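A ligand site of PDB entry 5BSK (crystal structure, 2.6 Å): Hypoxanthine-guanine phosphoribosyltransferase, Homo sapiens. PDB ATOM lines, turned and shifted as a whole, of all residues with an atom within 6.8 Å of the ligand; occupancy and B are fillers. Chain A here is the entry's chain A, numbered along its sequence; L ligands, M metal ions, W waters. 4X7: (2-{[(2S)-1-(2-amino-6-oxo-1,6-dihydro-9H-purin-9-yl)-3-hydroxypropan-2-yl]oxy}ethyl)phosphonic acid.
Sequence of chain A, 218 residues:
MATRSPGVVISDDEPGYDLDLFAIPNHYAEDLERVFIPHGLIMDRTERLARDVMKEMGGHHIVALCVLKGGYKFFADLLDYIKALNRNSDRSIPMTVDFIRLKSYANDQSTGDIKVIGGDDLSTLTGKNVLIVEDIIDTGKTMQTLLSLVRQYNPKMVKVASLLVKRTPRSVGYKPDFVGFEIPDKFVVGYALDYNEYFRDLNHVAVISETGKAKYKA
The side-chain hydroxyl (OG1) of Thr 142 lies within hydrogen-bond range of an oxygen (OAF) of the ligand (2.4 Å).
A nitrogen (N2) of the ligand sits at hydrogen-bond distance from the backbone carbonyl oxygen of Asp 194.
An oxygen (OAC) of the ligand lies within hydrogen-bond range of the backbone NH of Gly 140.
The side-chain amino group of Lys 166 lies within hydrogen-bond range of an oxygen (O6) of the ligand (3.2 Å).
OG1 of Thr 139 lies within hydrogen-bond range of OAE of the ligand (2.8 Å).
The backbone NH (N) of Thr 139 sits at hydrogen-bond distance from an oxygen (OAE) of the ligand (2.9 Å).
An oxygen (O6) of the ligand is in hydrogen-bond range of the backbone NH of Val 188 (3.1 Å).
An oxygen (OAF) of the ligand sits close to the backbone NH (N) of Thr 142 (3.2 Å).
O of Val 188 is in hydrogen-bond range of N1 of the ligand (2.9 Å).
N of Asp 138 lies within hydrogen-bond range of OAC of the ligand (3.2 Å).
Water W1 lies within hydrogen-bond range of OAE of the ligand and OD2 of Asp 138.
Ile 136 touches the ligand (CD1 to O6, 3.6 Å).
Ile 137 touches the ligand.
Lys 141 touches the ligand.
O of Lys 186 touches O6 of the ligand, at 3.7 Å.
CZ of Phe 187 touches C2 of the ligand, 3.4 Å away.
Leu 193 touches the ligand (CB to N2, 3.8 Å).
Hydrophobic or aromatic side chains within 4 Å of the ligand: Ile 136, Ile 137, Phe 187, Val 188 and Leu 193.
13 residues have an atom within 4 Å of the ligand: Ile 136, Ile 137, Asp 138, Thr 139, Gly 140, Lys 141, Thr 142, Lys 166, Lys 186, Phe 187, Val 188, Leu 193 and Asp 194.
The side-chain carboxylate (OD2) of Asp 138 is in salt-bridge range of the guanidinium group (NH1) of Arg 170 (2.6 Å).
The side-chain hydroxyl (OG1) of Thr 139 sits at hydrogen-bond distance from the backbone NH (N) of Lys 141 (3.3 Å).
The backbone NH of Ile 137 is in hydrogen-bond range of the backbone carbonyl oxygen of Leu 164, at 2.9 Å.
The side-chain amino group (NZ) of Lys 166 lies close to the backbone carbonyl oxygen (O) of Lys 186 (3.4 Å).
The backbone carbonyl oxygen (O) of Ile 137 lies within hydrogen-bond range of the backbone NH (N) of Lys 166 (3.2 Å).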
ATOM      1  N   LYS A  69      23.062  11.321  14.853  1.00  0.00           N
ATOM      2  CA  LYS A  69      24.368  10.892  14.368  1.00  0.00           C
ATOM      3  C   LYS A  69      24.807   9.580  15.003  1.00  0.00           C
ATOM      4  O   LYS A  69      24.362   9.223  16.098  1.00  0.00           O
ATOM      5  CB  LYS A  69      25.405  11.968  14.603  1.00  0.00           C
ATOM      6  N   GLY A  70      25.691   8.871  14.314  1.00  0.00           N
ATOM      7  CA  GLY A  70      26.171   7.583  14.777  1.00  0.00           C
ATOM      8  C   GLY A  70      25.611   6.451  13.940  1.00  0.00           C
ATOM      9  O   GLY A  70      24.405   6.253  13.888  1.00  0.00           O
ATOM     10  N   GLY A  71      26.503   5.721  13.272  1.00  0.00           N
ATOM     11  CA  GLY A  71      26.088   4.586  12.467  1.00  0.00           C
ATOM     12  C   GLY A  71      25.951   4.905  10.989  1.00  0.00           C
ATOM     13  O   GLY A  71      25.029   4.415  10.333  1.00  0.00           O
ATOM     14  N   GLU A 134      19.028   2.500  10.881  1.00  0.00           N
ATOM     15  CA  GLU A 134      19.632   2.812  12.161  1.00  0.00           C
ATOM     16  C   GLU A 134      20.714   1.786  12.496  1.00  0.00           C
ATOM     17  O   GLU A 134      20.630   0.635  12.082  1.00  0.00           O
ATOM     18  CB  GLU A 134      18.572   2.840  13.272  1.00  0.00           C
ATOM     19  CG  GLU A 134      19.083   3.240  14.637  1.00  0.00           C
ATOM     20  CD  GLU A 134      19.330   4.732  14.766  1.00  0.00           C
ATOM     21  OE1 GLU A 134      18.368   5.509  14.636  1.00  0.00           O
ATOM     22  OE2 GLU A 134      20.495   5.120  14.992  1.00  0.00           O
ATOM     23  N   ASP A 135      21.734   2.211  13.238  1.00  0.00           N
ATOM     24  CA  ASP A 135      22.814   1.313  13.628  1.00  0.00           C
ATOM     25  C   ASP A 135      22.417   0.441  14.802  1.00  0.00           C
ATOM     26  O   ASP A 135      22.557  -0.791  14.751  1.00  0.00           O
ATOM     27  CB  ASP A 135      24.073   2.115  13.969  1.00  0.00           C
ATOM     28  CG  ASP A 135      23.787   3.317  14.847  1.00  0.00           C
ATOM     29  OD1 ASP A 135      22.590   3.605  15.086  1.00  0.00           O
ATOM     30  OD2 ASP A 135      24.748   3.986  15.279  1.00  0.00           O
ATOM     31  N   ILE A 136      21.907   1.053  15.867  1.00  0.00           N
ATOM     32  CA  ILE A 136      21.511   0.315  17.050  1.00  0.00           C
ATOM     33  C   ILE A 136      20.235   0.877  17.675  1.00  0.00           C
ATOM     34  O   ILE A 136      20.020   2.091  17.698  1.00  0.00           O
ATOM     35  CB  ILE A 136      22.649   0.289  18.106  1.00  0.00           C
ATOM     36  CG1 ILE A 136      22.284  -0.631  19.280  1.00  0.00           C
ATOM     37  CG2 ILE A 136      22.970   1.698  18.595  1.00  0.00           C
ATOM     38  CD1 ILE A 136      23.360  -0.727  20.338  1.00  0.00           C
ATOM     39  N   ILE A 137      19.381  -0.015  18.154  1.00  0.00           N
ATOM     40  CA  ILE A 137      18.192   0.379  18.905  1.00  0.00           C
ATOM     41  C   ILE A 137      18.261  -0.227  20.302  1.00  0.00           C
ATOM     42  O   ILE A 137      18.210  -1.450  20.472  1.00  0.00           O
ATOM     43  CB  ILE A 137      16.898  -0.068  18.206  1.00  0.00           C
ATOM     44  CG1 ILE A 137      16.701   0.716  16.910  1.00  0.00           C
ATOM     45  CG2 ILE A 137      15.707   0.123  19.125  1.00  0.00           C
ATOM     46  CD1 ILE A 137      15.359   0.488  16.241  1.00  0.00           C
ATOM     47  N   ASP A 138      18.373   0.643  21.305  1.00  0.00           N
ATOM     48  CA  ASP A 138      18.451   0.209  22.694  1.00  0.00           C
ATOM     49  C   ASP A 138      17.059   0.178  23.310  1.00  0.00           C
ATOM     50  O   ASP A 138      16.391  -0.856  23.314  1.00  0.00           O
ATOM     51  CB  ASP A 138      19.385   1.117  23.492  1.00  0.00           C
ATOM     52  CG  ASP A 138      19.514   0.710  24.942  1.00  0.00           C
ATOM     53  OD1 ASP A 138      19.274  -0.472  25.256  1.00  0.00           O
ATOM     54  OD2 ASP A 138      19.858   1.569  25.777  1.00  0.00           O
ATOM     55  N   THR A 139      16.627   1.316  23.837  1.00  0.00           N
ATOM     56  CA  THR A 139      15.299   1.419  24.444  1.00  0.00           C
ATOM     57  C   THR A 139      14.214   1.419  23.363  1.00  0.00           C
ATOM     58  O   THR A 139      13.190   0.750  23.501  1.00  0.00           O
ATOM     59  CB  THR A 139      15.165   2.699  25.294  1.00  0.00           C
ATOM     60  OG1 THR A 139      15.387   3.850  24.474  1.00  0.00           O
ATOM     61  CG2 THR A 139      16.168   2.677  26.433  1.00  0.00           C
ATOM     62  N   GLY A 140      14.451   2.169  22.295  1.00  0.00           N
ATOM     63  CA  GLY A 140      13.500   2.267  21.203  1.00  0.00           C
ATOM     64  C   GLY A 140      12.818   3.631  21.164  1.00  0.00           C
ATOM     65  O   GLY A 140      11.969   3.873  20.303  1.00  0.00           O
ATOM     66  N   LYS A 141      13.199   4.499  22.089  1.00  0.00           N
ATOM     67  CA  LYS A 141      12.601   5.832  22.192  1.00  0.00           C
ATOM     68  C   LYS A 141      12.928   6.684  20.965  1.00  0.00           C
ATOM     69  O   LYS A 141      12.079   7.436  20.491  1.00  0.00           O
ATOM     70  CB  LYS A 141      13.071   6.523  23.458  1.00  0.00           C
ATOM     71  N   THR A 142      14.154   6.572  20.478  1.00  0.00           N
ATOM     72  CA  THR A 142      14.596   7.338  19.322  1.00  0.00           C
ATOM     73  C   THR A 142      13.767   7.006  18.085  1.00  0.00           C
ATOM     74  O   THR A 142      13.255   7.899  17.401  1.00  0.00           O
ATOM     75  CB  THR A 142      16.079   7.081  18.999  1.00  0.00           C
ATOM     76  OG1 THR A 142      16.892   7.458  20.118  1.00  0.00           O
ATOM     77  CG2 THR A 142      16.510   7.880  17.781  1.00  0.00           C
ATOM     78  N   MET A 143      13.625   5.716  17.807  1.00  0.00           N
ATOM     79  CA  MET A 143      12.894   5.267  16.629  1.00  0.00           C
ATOM     80  C   MET A 143      11.398   5.508  16.755  1.00  0.00           C
ATOM     81  O   MET A 143      10.722   5.762  15.761  1.00  0.00           O
ATOM     82  CB  MET A 143      13.167   3.776  16.368  1.00  0.00           C
ATOM     83  CG  MET A 143      12.771   3.325  14.976  1.00  0.00           C
ATOM     84  SD  MET A 143      13.568   4.280  13.687  1.00  0.00           S
ATOM     85  CE  MET A 143      15.287   4.070  14.123  1.00  0.00           C
ATOM     86  N   LEU A 164      21.725  -3.483  14.927  1.00  0.00           N
ATOM     87  CA  LEU A 164      21.747  -4.057  16.260  1.00  0.00           C
ATOM     88  C   LEU A 164      20.470  -3.750  17.043  1.00  0.00           C
ATOM     89  O   LEU A 164      19.917  -2.650  16.957  1.00  0.00           O
ATOM     90  CB  LEU A 164      22.954  -3.527  17.036  1.00  0.00           C
ATOM     91  CG  LEU A 164      24.316  -3.670  16.366  1.00  0.00           C
ATOM     92  CD1 LEU A 164      25.417  -3.120  17.271  1.00  0.00           C
ATOM     93  CD2 LEU A 164      24.589  -5.110  15.998  1.00  0.00           C
ATOM     94  N   LYS A 166      19.176  -4.404  21.114  1.00  0.00           N
ATOM     95  CA  LYS A 166      19.480  -4.903  22.453  1.00  0.00           C
ATOM     96  C   LYS A 166      18.317  -5.649  23.094  1.00  0.00           C
ATOM     97  O   LYS A 166      17.170  -5.199  23.025  1.00  0.00           O
ATOM     98  CB  LYS A 166      19.906  -3.759  23.369  1.00  0.00           C
ATOM     99  CG  LYS A 166      21.351  -3.337  23.249  1.00  0.00           C
ATOM    100  CD  LYS A 166      21.724  -2.403  24.395  1.00  0.00           C
ATOM    101  CE  LYS A 166      23.158  -1.940  24.285  1.00  0.00           C
ATOM    102  NZ  LYS A 166      23.541  -1.064  25.431  1.00  0.00           N
ATOM    103  N   ARG A 170      14.958  -2.147  29.434  1.00  0.00           N
ATOM    104  CA  ARG A 170      14.625  -0.744  29.230  1.00  0.00           C
ATOM    105  C   ARG A 170      13.839  -0.519  27.943  1.00  0.00           C
ATOM    106  O   ARG A 170      13.484   0.609  27.620  1.00  0.00           O
ATOM    107  CB  ARG A 170      15.900   0.105  29.213  1.00  0.00           C
ATOM    108  CG  ARG A 170      16.536   0.329  30.578  1.00  0.00           C
ATOM    109  CD  ARG A 170      17.833   1.112  30.473  1.00  0.00           C
ATOM    110  NE  ARG A 170      18.951   0.256  30.077  1.00  0.00           N
ATOM    111  CZ  ARG A 170      19.308   0.018  28.818  1.00  0.00           C
ATOM    112  NH1 ARG A 170      18.642   0.562  27.819  1.00  0.00           N
ATOM    113  NH2 ARG A 170      20.344  -0.775  28.562  1.00  0.00           N
ATOM    114  N   ILE A 183      21.624  -8.391  20.220  1.00  0.00           N
ATOM    115  CA  ILE A 183      22.744  -8.516  21.156  1.00  0.00           C
ATOM    116  C   ILE A 183      22.317  -8.374  22.619  1.00  0.00           C
ATOM    117  O   ILE A 183      21.278  -7.784  22.908  1.00  0.00           O
ATOM    118  CB  ILE A 183      23.830  -7.472  20.843  1.00  0.00           C
ATOM    119  CG1 ILE A 183      23.317  -6.051  21.106  1.00  0.00           C
ATOM    120  CG2 ILE A 183      24.317  -7.620  19.409  1.00  0.00           C
ATOM    121  CD1 ILE A 183      24.340  -4.974  20.849  1.00  0.00           C
ATOM    122  N   LYS A 186      24.607  -5.028  26.760  1.00  0.00           N
ATOM    123  CA  LYS A 186      25.934  -4.527  27.110  1.00  0.00           C
ATOM    124  C   LYS A 186      26.329  -3.389  26.174  1.00  0.00           C
ATOM    125  O   LYS A 186      25.960  -3.391  24.995  1.00  0.00           O
ATOM    126  CB  LYS A 186      26.976  -5.646  27.048  1.00  0.00           C
ATOM    127  CG  LYS A 186      26.500  -6.994  27.589  1.00  0.00           C
ATOM    128  CD  LYS A 186      27.496  -7.581  28.577  1.00  0.00           C
ATOM    129  CE  LYS A 186      27.548  -6.781  29.867  1.00  0.00           C
ATOM    130  NZ  LYS A 186      28.458  -7.396  30.867  1.00  0.00           N
ATOM    131  N   PHE A 187      27.061  -2.415  26.700  1.00  0.00           N
ATOM    132  CA  PHE A 187      27.498  -1.279  25.893  1.00  0.00           C
ATOM    133  C   PHE A 187      28.566  -1.720  24.895  1.00  0.00           C
ATOM    134  O   PHE A 187      29.663  -2.127  25.280  1.00  0.00           O
ATOM    135  CB  PHE A 187      28.041  -0.162  26.783  1.00  0.00           C
ATOM    136  CG  PHE A 187      28.173   1.160  26.088  1.00  0.00           C
ATOM    137  CD1 PHE A 187      29.298   1.463  25.341  1.00  0.00           C
ATOM    138  CD2 PHE A 187      27.166   2.112  26.183  1.00  0.00           C
ATOM    139  CE1 PHE A 187      29.415   2.677  24.698  1.00  0.00           C
ATOM    140  CE2 PHE A 187      27.284   3.333  25.552  1.00  0.00           C
ATOM    141  CZ  PHE A 187      28.408   3.612  24.804  1.00  0.00           C
ATOM    142  N   VAL A 188      28.243  -1.624  23.607  1.00  0.00           N
ATOM    143  CA  VAL A 188      29.156  -2.064  22.555  1.00  0.00           C
ATOM    144  C   VAL A 188      29.716  -0.891  21.750  1.00  0.00           C
ATOM    145  O   VAL A 188      29.094   0.160  21.645  1.00  0.00           O
ATOM    146  CB  VAL A 188      28.464  -3.048  21.594  1.00  0.00           C
ATOM    147  CG1 VAL A 188      28.103  -4.328  22.321  1.00  0.00           C
ATOM    148  CG2 VAL A 188      27.224  -2.409  20.977  1.00  0.00           C
ATOM    149  N   VAL A 189      30.907  -1.099  21.185  1.00  0.00           N
ATOM    150  CA  VAL A 189      31.529  -0.104  20.322  1.00  0.00           C
ATOM    151  C   VAL A 189      32.125  -0.782  19.093  1.00  0.00           C
ATOM    152  O   VAL A 189      32.296  -2.009  19.068  1.00  0.00           O
ATOM    153  CB  VAL A 189      32.640   0.678  21.049  1.00  0.00           C
ATOM    154  CG1 VAL A 189      32.050   1.582  22.129  1.00  0.00           C
ATOM    155  CG2 VAL A 189      33.667  -0.270  21.644  1.00  0.00           C
ATOM    156  N   GLY A 190      32.432   0.006  18.067  1.00  0.00           N
ATOM    157  CA  GLY A 190      33.062  -0.525  16.868  1.00  0.00           C
ATOM    158  C   GLY A 190      32.178  -0.498  15.642  1.00  0.00           C
ATOM    159  O   GLY A 190      30.962  -0.282  15.745  1.00  0.00           O
ATOM    160  N   LEU A 193      29.522   2.173  15.646  1.00  0.00           N
ATOM    161  CA  LEU A 193      29.286   2.799  16.942  1.00  0.00           C
ATOM    162  C   LEU A 193      30.577   3.349  17.543  1.00  0.00           C
ATOM    163  O   LEU A 193      31.575   2.633  17.639  1.00  0.00           O
ATOM    164  CB  LEU A 193      28.638   1.804  17.900  1.00  0.00           C
ATOM    165  CG  LEU A 193      27.266   1.273  17.465  1.00  0.00           C
ATOM    166  CD1 LEU A 193      26.717   0.289  18.478  1.00  0.00           C
ATOM    167  CD2 LEU A 193      26.299   2.435  17.272  1.00  0.00           C
ATOM    168  N   ASP A 194      30.538   4.608  17.941  1.00  0.00           N
ATOM    169  CA  ASP A 194      31.693   5.258  18.550  1.00  0.00           C
ATOM    170  C   ASP A 194      31.427   5.606  20.005  1.00  0.00           C
ATOM    171  O   ASP A 194      30.278   5.650  20.439  1.00  0.00           O
ATOM    172  CB  ASP A 194      32.062   6.515  17.770  1.00  0.00           C
ATOM    173  CG  ASP A 194      31.111   7.659  18.022  1.00  0.00           C
ATOM    174  OD1 ASP A 194      30.023   7.687  17.386  1.00  0.00           O
ATOM    175  OD2 ASP A 194      31.420   8.541  18.856  1.00  0.00           O
ATOM    176  N   TYR A 195      32.501   5.851  20.759  1.00  0.00           N
ATOM    177  CA  TYR A 195      32.384   6.305  22.136  1.00  0.00           C
ATOM    178  C   TYR A 195      33.177   7.594  22.299  1.00  0.00           C
ATOM    179  O   TYR A 195      34.404   7.559  22.410  1.00  0.00           O
ATOM    180  CB  TYR A 195      32.873   5.240  23.114  1.00  0.00           C
ATOM    181  CG  TYR A 195      32.708   5.623  24.566  1.00  0.00           C
ATOM    182  CD1 TYR A 195      31.496   5.437  25.219  1.00  0.00           C
ATOM    183  CD2 TYR A 195      33.755   6.175  25.285  1.00  0.00           C
ATOM    184  CE1 TYR A 195      31.330   5.787  26.542  1.00  0.00           C
ATOM    185  CE2 TYR A 195      33.605   6.531  26.618  1.00  0.00           C
ATOM    186  CZ  TYR A 195      32.395   6.327  27.240  1.00  0.00           C
ATOM    187  OH  TYR A 195      32.238   6.688  28.563  1.00  0.00           O
HETATM  188  C4  4X7 L   1      24.601   3.308  22.480  1.00  0.00           C
HETATM  189  C5  4X7 L   1      24.497   1.976  22.894  1.00  0.00           C
HETATM  190  C6  4X7 L   1      25.585   1.140  22.758  1.00  0.00           C
HETATM  191  C8  4X7 L   1      22.533   3.013  23.261  1.00  0.00           C
HETATM  192  N1  4X7 L   1      26.723   1.656  22.221  1.00  0.00           N
HETATM  193  N2  4X7 L   1      28.033   3.451  21.261  1.00  0.00           N
HETATM  194  N3  4X7 L   1      25.820   3.770  21.932  1.00  0.00           N
HETATM  195  OAE 4X7 L   1      17.862   3.908  23.214  1.00  0.00           O
HETATM  196  PAV 4X7 L   1      17.587   4.285  21.812  1.00  0.00           P
HETATM  197  OAF 4X7 L   1      16.988   5.704  21.787  1.00  0.00           O
HETATM  198  OAC 4X7 L   1      16.614   3.328  21.218  1.00  0.00           O
HETATM  199  CAJ 4X7 L   1      19.138   4.245  20.833  1.00  0.00           C
HETATM  200  CAI 4X7 L   1      20.278   4.863  21.599  1.00  0.00           C
HETATM  201  OAO 4X7 L   1      21.439   4.844  20.770  1.00  0.00           O
HETATM  202  CAT 4X7 L   1      22.523   5.627  21.081  1.00  0.00           C
HETATM  203  CAH 4X7 L   1      23.569   5.421  20.007  1.00  0.00           C
HETATM  204  OAD 4X7 L   1      23.160   5.557  18.690  1.00  0.00           O
HETATM  205  CAK 4X7 L   1      23.032   5.288  22.451  1.00  0.00           C
HETATM  206  N9  4X7 L   1      23.360   3.915  22.721  1.00  0.00           N
HETATM  207  C2  4X7 L   1      26.814   2.980  21.814  1.00  0.00           C
HETATM  208  O6  4X7 L   1      25.523  -0.169  23.151  1.00  0.00           O
HETATM  209  N7  4X7 L   1      23.211   1.813  23.374  1.00  0.00           N
HETATM  210 MG    MG M   1      22.426   5.763  15.322  1.00  0.00          MG
HETATM  211  O   HOH W   1      19.390   4.022  25.084  1.00  0.00           O
